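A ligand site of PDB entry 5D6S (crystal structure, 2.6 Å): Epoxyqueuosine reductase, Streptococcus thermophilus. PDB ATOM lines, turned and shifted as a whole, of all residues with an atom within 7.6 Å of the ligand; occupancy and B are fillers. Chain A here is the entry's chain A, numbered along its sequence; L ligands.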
ATOM      1  N   PHE A 174      17.053   3.730   8.424  1.00  0.00           N
ATOM      2  CA  PHE A 174      16.032   4.273   9.305  1.00  0.00           C
ATOM      3  C   PHE A 174      16.584   4.431  10.733  1.00  0.00           C
ATOM      4  O   PHE A 174      17.583   3.792  11.108  1.00  0.00           O
ATOM      5  CB  PHE A 174      14.817   3.364   9.341  1.00  0.00           C
ATOM      6  CG  PHE A 174      15.029   2.088  10.106  1.00  0.00           C
ATOM      7  CD1 PHE A 174      15.768   1.031   9.573  1.00  0.00           C
ATOM      8  CD2 PHE A 174      14.463   1.927  11.374  1.00  0.00           C
ATOM      9  CE1 PHE A 174      15.939  -0.160  10.274  1.00  0.00           C
ATOM     10  CE2 PHE A 174      14.638   0.749  12.076  1.00  0.00           C
ATOM     11  CZ  PHE A 174      15.377  -0.299  11.520  1.00  0.00           C
ATOM     12  N   ILE A 175      15.932   5.287  11.525  1.00  0.00           N
ATOM     13  CA  ILE A 175      16.349   5.495  12.877  1.00  0.00           C
ATOM     14  C   ILE A 175      15.623   4.468  13.737  1.00  0.00           C
ATOM     15  O   ILE A 175      14.394   4.452  13.795  1.00  0.00           O
ATOM     16  CB  ILE A 175      16.086   6.940  13.335  1.00  0.00           C
ATOM     17  CG1 ILE A 175      17.141   7.865  12.735  1.00  0.00           C
ATOM     18  CG2 ILE A 175      16.095   7.074  14.851  1.00  0.00           C
ATOM     19  CD1 ILE A 175      16.857   9.333  12.892  1.00  0.00           C
ATOM     20  N   GLY A 176      16.394   3.635  14.434  1.00  0.00           N
ATOM     21  CA  GLY A 176      15.822   2.681  15.364  1.00  0.00           C
ATOM     22  C   GLY A 176      15.257   3.304  16.634  1.00  0.00           C
ATOM     23  O   GLY A 176      15.349   4.501  16.864  1.00  0.00           O
ATOM     24  N   LYS A 177      14.655   2.461  17.468  1.00  0.00           N
ATOM     25  CA  LYS A 177      14.246   2.856  18.816  1.00  0.00           C
ATOM     26  C   LYS A 177      15.489   3.073  19.691  1.00  0.00           C
ATOM     27  O   LYS A 177      15.434   3.753  20.734  1.00  0.00           O
ATOM     28  CB  LYS A 177      13.318   1.798  19.443  1.00  0.00           C
ATOM     29  CG  LYS A 177      11.907   1.721  18.845  1.00  0.00           C
ATOM     30  CD  LYS A 177      11.269   0.354  19.081  1.00  0.00           C
ATOM     31  CE  LYS A 177       9.760   0.413  19.205  1.00  0.00           C
ATOM     32  NZ  LYS A 177       9.176  -0.956  19.282  1.00  0.00           N
ATOM     33  N   ASN A 178      16.620   2.468  19.283  1.00  0.00           N
ATOM     34  CA  ASN A 178      17.902   2.659  19.969  1.00  0.00           C
ATOM     35  C   ASN A 178      18.573   3.977  19.601  1.00  0.00           C
ATOM     36  O   ASN A 178      19.650   4.276  20.098  1.00  0.00           O
ATOM     37  CB  ASN A 178      18.842   1.475  19.739  1.00  0.00           C
ATOM     38  CG  ASN A 178      19.357   1.399  18.315  1.00  0.00           C
ATOM     39  OD1 ASN A 178      19.107   2.273  17.489  1.00  0.00           O
ATOM     40  ND2 ASN A 178      20.066   0.311  18.011  1.00  0.00           N
ATOM     41  N   GLY A 179      17.962   4.758  18.721  1.00  0.00           N
ATOM     42  CA  GLY A 179      18.466   6.079  18.360  1.00  0.00           C
ATOM     43  C   GLY A 179      19.407   6.072  17.172  1.00  0.00           C
ATOM     44  O   GLY A 179      19.706   7.115  16.593  1.00  0.00           O
ATOM     45  N   LEU A 180      19.851   4.891  16.774  1.00  0.00           N
ATOM     46  CA  LEU A 180      20.843   4.771  15.713  1.00  0.00           C
ATOM     47  C   LEU A 180      20.264   4.599  14.307  1.00  0.00           C
ATOM     48  O   LEU A 180      19.120   4.201  14.126  1.00  0.00           O
ATOM     49  CB  LEU A 180      21.755   3.583  16.019  1.00  0.00           C
ATOM     50  CG  LEU A 180      22.644   3.750  17.242  1.00  0.00           C
ATOM     51  CD1 LEU A 180      23.207   2.390  17.661  1.00  0.00           C
ATOM     52  CD2 LEU A 180      23.771   4.717  16.937  1.00  0.00           C
ATOM     53  N   ILE A 182      20.057   2.548  11.033  1.00  0.00           N
ATOM     54  CA  ILE A 182      20.127   1.123  10.685  1.00  0.00           C
ATOM     55  C   ILE A 182      19.905   0.933   9.190  1.00  0.00           C
ATOM     56  O   ILE A 182      18.859   1.320   8.653  1.00  0.00           O
ATOM     57  CB  ILE A 182      18.998   0.323  11.378  1.00  0.00           C
ATOM     58  CG1 ILE A 182      18.803   0.729  12.855  1.00  0.00           C
ATOM     59  CG2 ILE A 182      19.217  -1.166  11.170  1.00  0.00           C
ATOM     60  CD1 ILE A 182      19.331  -0.235  13.898  1.00  0.00           C
ATOM     61  N   SER A 188      23.508  -1.350  11.858  1.00  0.00           N
ATOM     62  CA  SER A 188      23.864  -0.044  12.454  1.00  0.00           C
ATOM     63  C   SER A 188      25.364   0.175  12.489  1.00  0.00           C
ATOM     64  O   SER A 188      25.811   1.298  12.708  1.00  0.00           O
ATOM     65  CB  SER A 188      23.283   0.115  13.854  1.00  0.00           C
ATOM     66  OG  SER A 188      23.339  -1.092  14.576  1.00  0.00           O
ATOM     67  N   GLY A 210      11.480  -0.700   9.083  1.00  0.00           N
ATOM     68  CA  GLY A 210      11.593  -0.036  10.367  1.00  0.00           C
ATOM     69  C   GLY A 210      11.794  -1.022  11.505  1.00  0.00           C
ATOM     70  O   GLY A 210      12.357  -2.113  11.319  1.00  0.00           O
ATOM     71  N   CYS A 211      11.306  -0.644  12.685  1.00  0.00           N
ATOM     72  CA  CYS A 211      11.450  -1.472  13.871  1.00  0.00           C
ATOM     73  C   CYS A 211      10.314  -2.487  14.018  1.00  0.00           C
ATOM     74  O   CYS A 211      10.540  -3.688  14.248  1.00  0.00           O
ATOM     75  CB  CYS A 211      11.518  -0.575  15.131  1.00  0.00           C
ATOM     76  SG  CYS A 211      13.170   0.068  15.518  1.00  0.00           S
ATOM     77  N   GLY A 212       9.087  -2.007  13.855  1.00  0.00           N
ATOM     78  CA  GLY A 212       7.906  -2.796  14.094  1.00  0.00           C
ATOM     79  C   GLY A 212       7.566  -2.669  15.553  1.00  0.00           C
ATOM     80  O   GLY A 212       7.432  -1.560  16.061  1.00  0.00           O
ATOM     81  N   ASP A 213       7.366  -3.801  16.210  1.00  0.00           N
ATOM     82  CA  ASP A 213       7.130  -3.828  17.653  1.00  0.00           C
ATOM     83  C   ASP A 213       8.274  -4.597  18.306  1.00  0.00           C
ATOM     84  O   ASP A 213       8.014  -5.507  19.088  1.00  0.00           O
ATOM     85  N   CYS A 214       9.525  -4.238  17.977  1.00  0.00           N
ATOM     86  CA  CYS A 214      10.711  -5.051  18.358  1.00  0.00           C
ATOM     87  C   CYS A 214      11.203  -4.927  19.804  1.00  0.00           C
ATOM     88  O   CYS A 214      11.356  -5.955  20.481  1.00  0.00           O
ATOM     89  CB  CYS A 214      11.882  -4.813  17.424  1.00  0.00           C
ATOM     90  SG  CYS A 214      13.410  -5.632  17.988  1.00  0.00           S
ATOM     91  N   ARG A 215      11.479  -3.722  20.271  1.00  0.00           N
ATOM     92  CA  ARG A 215      11.766  -3.505  21.701  1.00  0.00           C
ATOM     93  C   ARG A 215      12.974  -4.228  22.336  1.00  0.00           C
ATOM     94  O   ARG A 215      13.119  -4.206  23.549  1.00  0.00           O
ATOM     95  CB  ARG A 215      10.535  -3.892  22.557  1.00  0.00           C
ATOM     96  CG  ARG A 215       9.474  -2.817  22.672  1.00  0.00           C
ATOM     97  CD  ARG A 215       8.495  -3.108  23.807  1.00  0.00           C
ATOM     98  NE  ARG A 215       9.202  -3.344  25.069  1.00  0.00           N
ATOM     99  CZ  ARG A 215       9.497  -2.415  25.968  1.00  0.00           C
ATOM    100  NH1 ARG A 215       9.173  -1.140  25.798  1.00  0.00           N
ATOM    101  NH2 ARG A 215      10.137  -2.770  27.072  1.00  0.00           N
ATOM    102  N   ARG A 216      13.808  -4.914  21.554  1.00  0.00           N
ATOM    103  CA  ARG A 216      14.890  -5.720  22.150  1.00  0.00           C
ATOM    104  C   ARG A 216      15.931  -4.845  22.872  1.00  0.00           C
ATOM    105  O   ARG A 216      16.319  -5.110  24.021  1.00  0.00           O
ATOM    106  CB  ARG A 216      15.590  -6.587  21.099  1.00  0.00           C
ATOM    107  CG  ARG A 216      14.805  -7.824  20.665  1.00  0.00           C
ATOM    108  CD  ARG A 216      15.721  -9.036  20.560  1.00  0.00           C
ATOM    109  NE  ARG A 216      15.537  -9.799  19.326  1.00  0.00           N
ATOM    110  CZ  ARG A 216      16.512 -10.396  18.643  1.00  0.00           C
ATOM    111  NH1 ARG A 216      16.231 -11.064  17.516  1.00  0.00           N
ATOM    112  NH2 ARG A 216      17.789 -10.338  19.046  1.00  0.00           N
ATOM    113  N   CYS A 217      16.386  -3.810  22.157  1.00  0.00           N
ATOM    114  CA  CYS A 217      17.306  -2.801  22.656  1.00  0.00           C
ATOM    115  C   CYS A 217      16.780  -2.154  23.936  1.00  0.00           C
ATOM    116  O   CYS A 217      17.471  -2.080  24.941  1.00  0.00           O
ATOM    117  CB  CYS A 217      17.535  -1.737  21.570  1.00  0.00           C
ATOM    118  SG  CYS A 217      16.025  -0.970  20.872  1.00  0.00           S
ATOM    119  N   LEU A 218      15.534  -1.697  23.904  1.00  0.00           N
ATOM    120  CA  LEU A 218      14.930  -1.109  25.113  1.00  0.00           C
ATOM    121  C   LEU A 218      15.007  -1.985  26.368  1.00  0.00           C
ATOM    122  O   LEU A 218      15.024  -1.466  27.462  1.00  0.00           O
ATOM    123  CB  LEU A 218      13.449  -0.816  24.876  1.00  0.00           C
ATOM    124  CG  LEU A 218      13.086   0.478  24.155  1.00  0.00           C
ATOM    125  CD1 LEU A 218      13.873   0.655  22.877  1.00  0.00           C
ATOM    126  CD2 LEU A 218      11.587   0.473  23.879  1.00  0.00           C
ATOM    127  N   LEU A 226      17.315   4.379  27.222  1.00  0.00           N
ATOM    128  CA  LEU A 226      16.504   4.544  26.004  1.00  0.00           C
ATOM    129  C   LEU A 226      15.031   4.743  26.360  1.00  0.00           C
ATOM    130  O   LEU A 226      14.489   4.001  27.166  1.00  0.00           O
ATOM    131  CB  LEU A 226      16.643   3.319  25.110  1.00  0.00           C
ATOM    132  CG  LEU A 226      18.040   3.142  24.536  1.00  0.00           C
ATOM    133  CD1 LEU A 226      18.291   1.732  24.043  1.00  0.00           C
ATOM    134  CD2 LEU A 226      18.305   4.142  23.421  1.00  0.00           C
ATOM    135  N   GLY A 228      12.243   4.997  24.272  1.00  0.00           N
ATOM    136  CA  GLY A 228      11.297   4.222  23.461  1.00  0.00           C
ATOM    137  C   GLY A 228      11.119   4.722  22.037  1.00  0.00           C
ATOM    138  O   GLY A 228      10.935   3.929  21.114  1.00  0.00           O
ATOM    139  N   ILE A 265      25.585  -2.750  23.537  1.00  0.00           N
ATOM    140  CA  ILE A 265      24.512  -3.658  23.934  1.00  0.00           C
ATOM    141  C   ILE A 265      23.231  -3.437  23.082  1.00  0.00           C
ATOM    142  O   ILE A 265      22.590  -4.396  22.683  1.00  0.00           O
ATOM    143  CB  ILE A 265      24.289  -3.567  25.475  1.00  0.00           C
ATOM    144  CG1 ILE A 265      25.506  -4.214  26.182  1.00  0.00           C
ATOM    145  CG2 ILE A 265      23.011  -4.268  25.936  1.00  0.00           C
ATOM    146  CD1 ILE A 265      25.687  -3.844  27.646  1.00  0.00           C
ATOM    147  N   CYS A 266      22.882  -2.186  22.812  1.00  0.00           N
ATOM    148  CA  CYS A 266      21.633  -1.840  22.082  1.00  0.00           C
ATOM    149  C   CYS A 266      21.745  -2.113  20.587  1.00  0.00           C
ATOM    150  O   CYS A 266      20.757  -1.990  19.865  1.00  0.00           O
ATOM    151  CB  CYS A 266      21.236  -0.376  22.331  1.00  0.00           C
ATOM    152  SG  CYS A 266      22.548   0.879  22.190  1.00  0.00           S
ATOM    153  N   GLN A 267      22.929  -2.494  20.137  1.00  0.00           N
ATOM    154  CA  GLN A 267      23.169  -2.905  18.750  1.00  0.00           C
ATOM    155  C   GLN A 267      23.362  -4.425  18.591  1.00  0.00           C
ATOM    156  O   GLN A 267      22.889  -5.022  17.629  1.00  0.00           O
ATOM    157  CB  GLN A 267      24.417  -2.205  18.206  1.00  0.00           C
ATOM    158  CG  GLN A 267      24.246  -0.713  17.908  1.00  0.00           C
ATOM    159  CD  GLN A 267      25.555  -0.061  17.458  1.00  0.00           C
ATOM    160  OE1 GLN A 267      26.360   0.365  18.291  1.00  0.00           O
ATOM    161  NE2 GLN A 267      25.760   0.036  16.160  1.00  0.00           N
ATOM    162  N   ILE A 268      24.102  -5.036  19.513  1.00  0.00           N
ATOM    163  CA  ILE A 268      24.234  -6.472  19.579  1.00  0.00           C
ATOM    164  C   ILE A 268      22.850  -7.142  19.699  1.00  0.00           C
ATOM    165  O   ILE A 268      22.603  -8.201  19.118  1.00  0.00           O
ATOM    166  CB  ILE A 268      25.147  -6.878  20.762  1.00  0.00           C
ATOM    167  CG1 ILE A 268      26.603  -6.565  20.426  1.00  0.00           C
ATOM    168  CG2 ILE A 268      24.989  -8.367  21.103  1.00  0.00           C
ATOM    169  CD1 ILE A 268      27.550  -6.639  21.604  1.00  0.00           C
ATOM    170  N   SER A 269      21.944  -6.519  20.457  1.00  0.00           N
ATOM    171  CA  SER A 269      20.599  -7.049  20.648  1.00  0.00           C
ATOM    172  C   SER A 269      19.660  -6.761  19.460  1.00  0.00           C
ATOM    173  O   SER A 269      18.493  -7.156  19.504  1.00  0.00           O
ATOM    174  CB  SER A 269      19.980  -6.483  21.936  1.00  0.00           C
ATOM    175  OG  SER A 269      19.451  -5.153  21.750  1.00  0.00           O
ATOM    176  N   CYS A 270      20.138  -6.089  18.405  1.00  0.00           N
ATOM    177  CA  CYS A 270      19.285  -5.677  17.290  1.00  0.00           C
ATOM    178  C   CYS A 270      19.238  -6.731  16.189  1.00  0.00           C
ATOM    179  O   CYS A 270      20.287  -7.146  15.684  1.00  0.00           O
ATOM    180  CB  CYS A 270      19.730  -4.346  16.689  1.00  0.00           C
ATOM    181  SG  CYS A 270      18.559  -3.650  15.471  1.00  0.00           S
ATOM    182  N   PRO A 271      18.011  -7.150  15.800  1.00  0.00           N
ATOM    183  CA  PRO A 271      17.795  -8.135  14.748  1.00  0.00           C
ATOM    184  C   PRO A 271      18.544  -7.804  13.473  1.00  0.00           C
ATOM    185  O   PRO A 271      19.145  -8.692  12.879  1.00  0.00           O
ATOM    186  CB  PRO A 271      16.296  -8.028  14.475  1.00  0.00           C
ATOM    187  CG  PRO A 271      15.710  -7.556  15.763  1.00  0.00           C
ATOM    188  CD  PRO A 271      16.738  -6.648  16.358  1.00  0.00           C
ATOM    189  N   TYR A 272      18.546  -6.530  13.086  1.00  0.00           N
ATOM    190  CA  TYR A 272      19.225  -6.118  11.856  1.00  0.00           C
ATOM    191  C   TYR A 272      20.724  -6.353  11.870  1.00  0.00           C
ATOM    192  O   TYR A 272      21.367  -6.252  10.818  1.00  0.00           O
ATOM    193  CB  TYR A 272      18.969  -4.664  11.540  1.00  0.00           C
ATOM    194  CG  TYR A 272      17.587  -4.355  11.072  1.00  0.00           C
ATOM    195  CD1 TYR A 272      16.553  -4.115  11.978  1.00  0.00           C
ATOM    196  CD2 TYR A 272      17.285  -4.301   9.702  1.00  0.00           C
ATOM    197  CE1 TYR A 272      15.263  -3.809  11.539  1.00  0.00           C
ATOM    198  CE2 TYR A 272      16.001  -4.018   9.245  1.00  0.00           C
ATOM    199  CZ  TYR A 272      15.005  -3.754  10.159  1.00  0.00           C
ATOM    200  OH  TYR A 272      13.756  -3.460   9.694  1.00  0.00           O
ATOM    201  N   ASN A 273      21.293  -6.628  13.036  1.00  0.00           N
ATOM    202  CA  ASN A 273      22.735  -6.930  13.142  1.00  0.00           C
ATOM    203  C   ASN A 273      23.003  -8.436  13.220  1.00  0.00           C
ATOM    204  O   ASN A 273      24.151  -8.869  13.131  1.00  0.00           O
ATOM    205  CB  ASN A 273      23.372  -6.175  14.316  1.00  0.00           C
ATOM    206  CG  ASN A 273      23.484  -4.669  14.065  1.00  0.00           C
ATOM    207  OD1 ASN A 273      23.968  -4.246  13.020  1.00  0.00           O
ATOM    208  ND2 ASN A 273      23.031  -3.850  15.024  1.00  0.00           N
HETATM  209 FE1  LIG L   1      15.792  -1.711  18.699  1.00  0.00          FE
HETATM  210 FE2  LIG L   1      14.740  -3.711  17.425  1.00  0.00          FE
HETATM  211 FE3  LIG L   1      16.924  -2.729  16.617  1.00  0.00          FE
HETATM  212 FE4  LIG L   1      14.662  -1.445  16.434  1.00  0.00          FE
HETATM  213  S1  LIG L   1      15.257  -3.166  15.408  1.00  0.00           S
HETATM  214  S2  LIG L   1      16.557  -0.707  17.013  1.00  0.00           S
HETATM  215  S3  LIG L   1      13.755  -2.044  18.281  1.00  0.00           S
HETATM  216  S4  LIG L   1      16.572  -3.640  18.453  1.00  0.00           S
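Gly 176 touches the ligand (CA to S2, 3.8 Å). Pro 271 touches the ligand. Tyr 272 touches the ligand (CD1 to S1, 3.8 Å). Hydrophobic or aromatic side chains within 4 Å of the ligand: Pro 271 and Tyr 272. Of the 29 residues printed, 10 come within 4 Å of the ligand.
S3 of the ligand lies close to N of Arg 215. The side-chain sulfur of Cys 214 is bound to an iron atom (FE2) of the ligand, 2.4 Å away. SG of Cys 270 binds FE3 of the ligand (2.2 Å). FE1 of the ligand is bound by SG of Cys 217, 2.3 Å away. ND2 of Asn 178 lies close to S2 of the ligand. An iron atom (FE4) of the ligand is bound by the side-chain sulfur (SG) of Cys 211, at 2.3 Å. S4 of the ligand sits close to N of Cys 217, 3.7 Å away. A sulfur (S2) of the ligand lies close to the backbone NH (N) of Lys 177 (3.7 Å).
The side-chain sulfur (SG) of Cys 270 sits close to the backbone NH (N) of Tyr 272 (3.7 Å). OD1 of Asn 178 lies within hydrogen-bond range of N of Leu 180 (2.8 Å). The backbone NH (N) of Arg 216 lies close to the side-chain sulfur (SG) of Cys 214, at 3.7 Å. The backbone NH (N) of Lys 177 sits close to the side-chain sulfur (SG) of Cys 211 (3.4 Å). The backbone NH (N) of Cys 217 lies close to the side-chain hydroxyl (OG) of Ser 269 (3.4 Å). The backbone carbonyl oxygen (O) of Gly 210 lies within hydrogen-bond range of the side-chain hydroxyl (OH) of Tyr 272, 2.5 Å away. The side-chain amide nitrogen (ND2) of Asn 178 sits at hydrogen-bond distance from the backbone carbonyl oxygen (O) of Cys 266 (3.0 Å).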
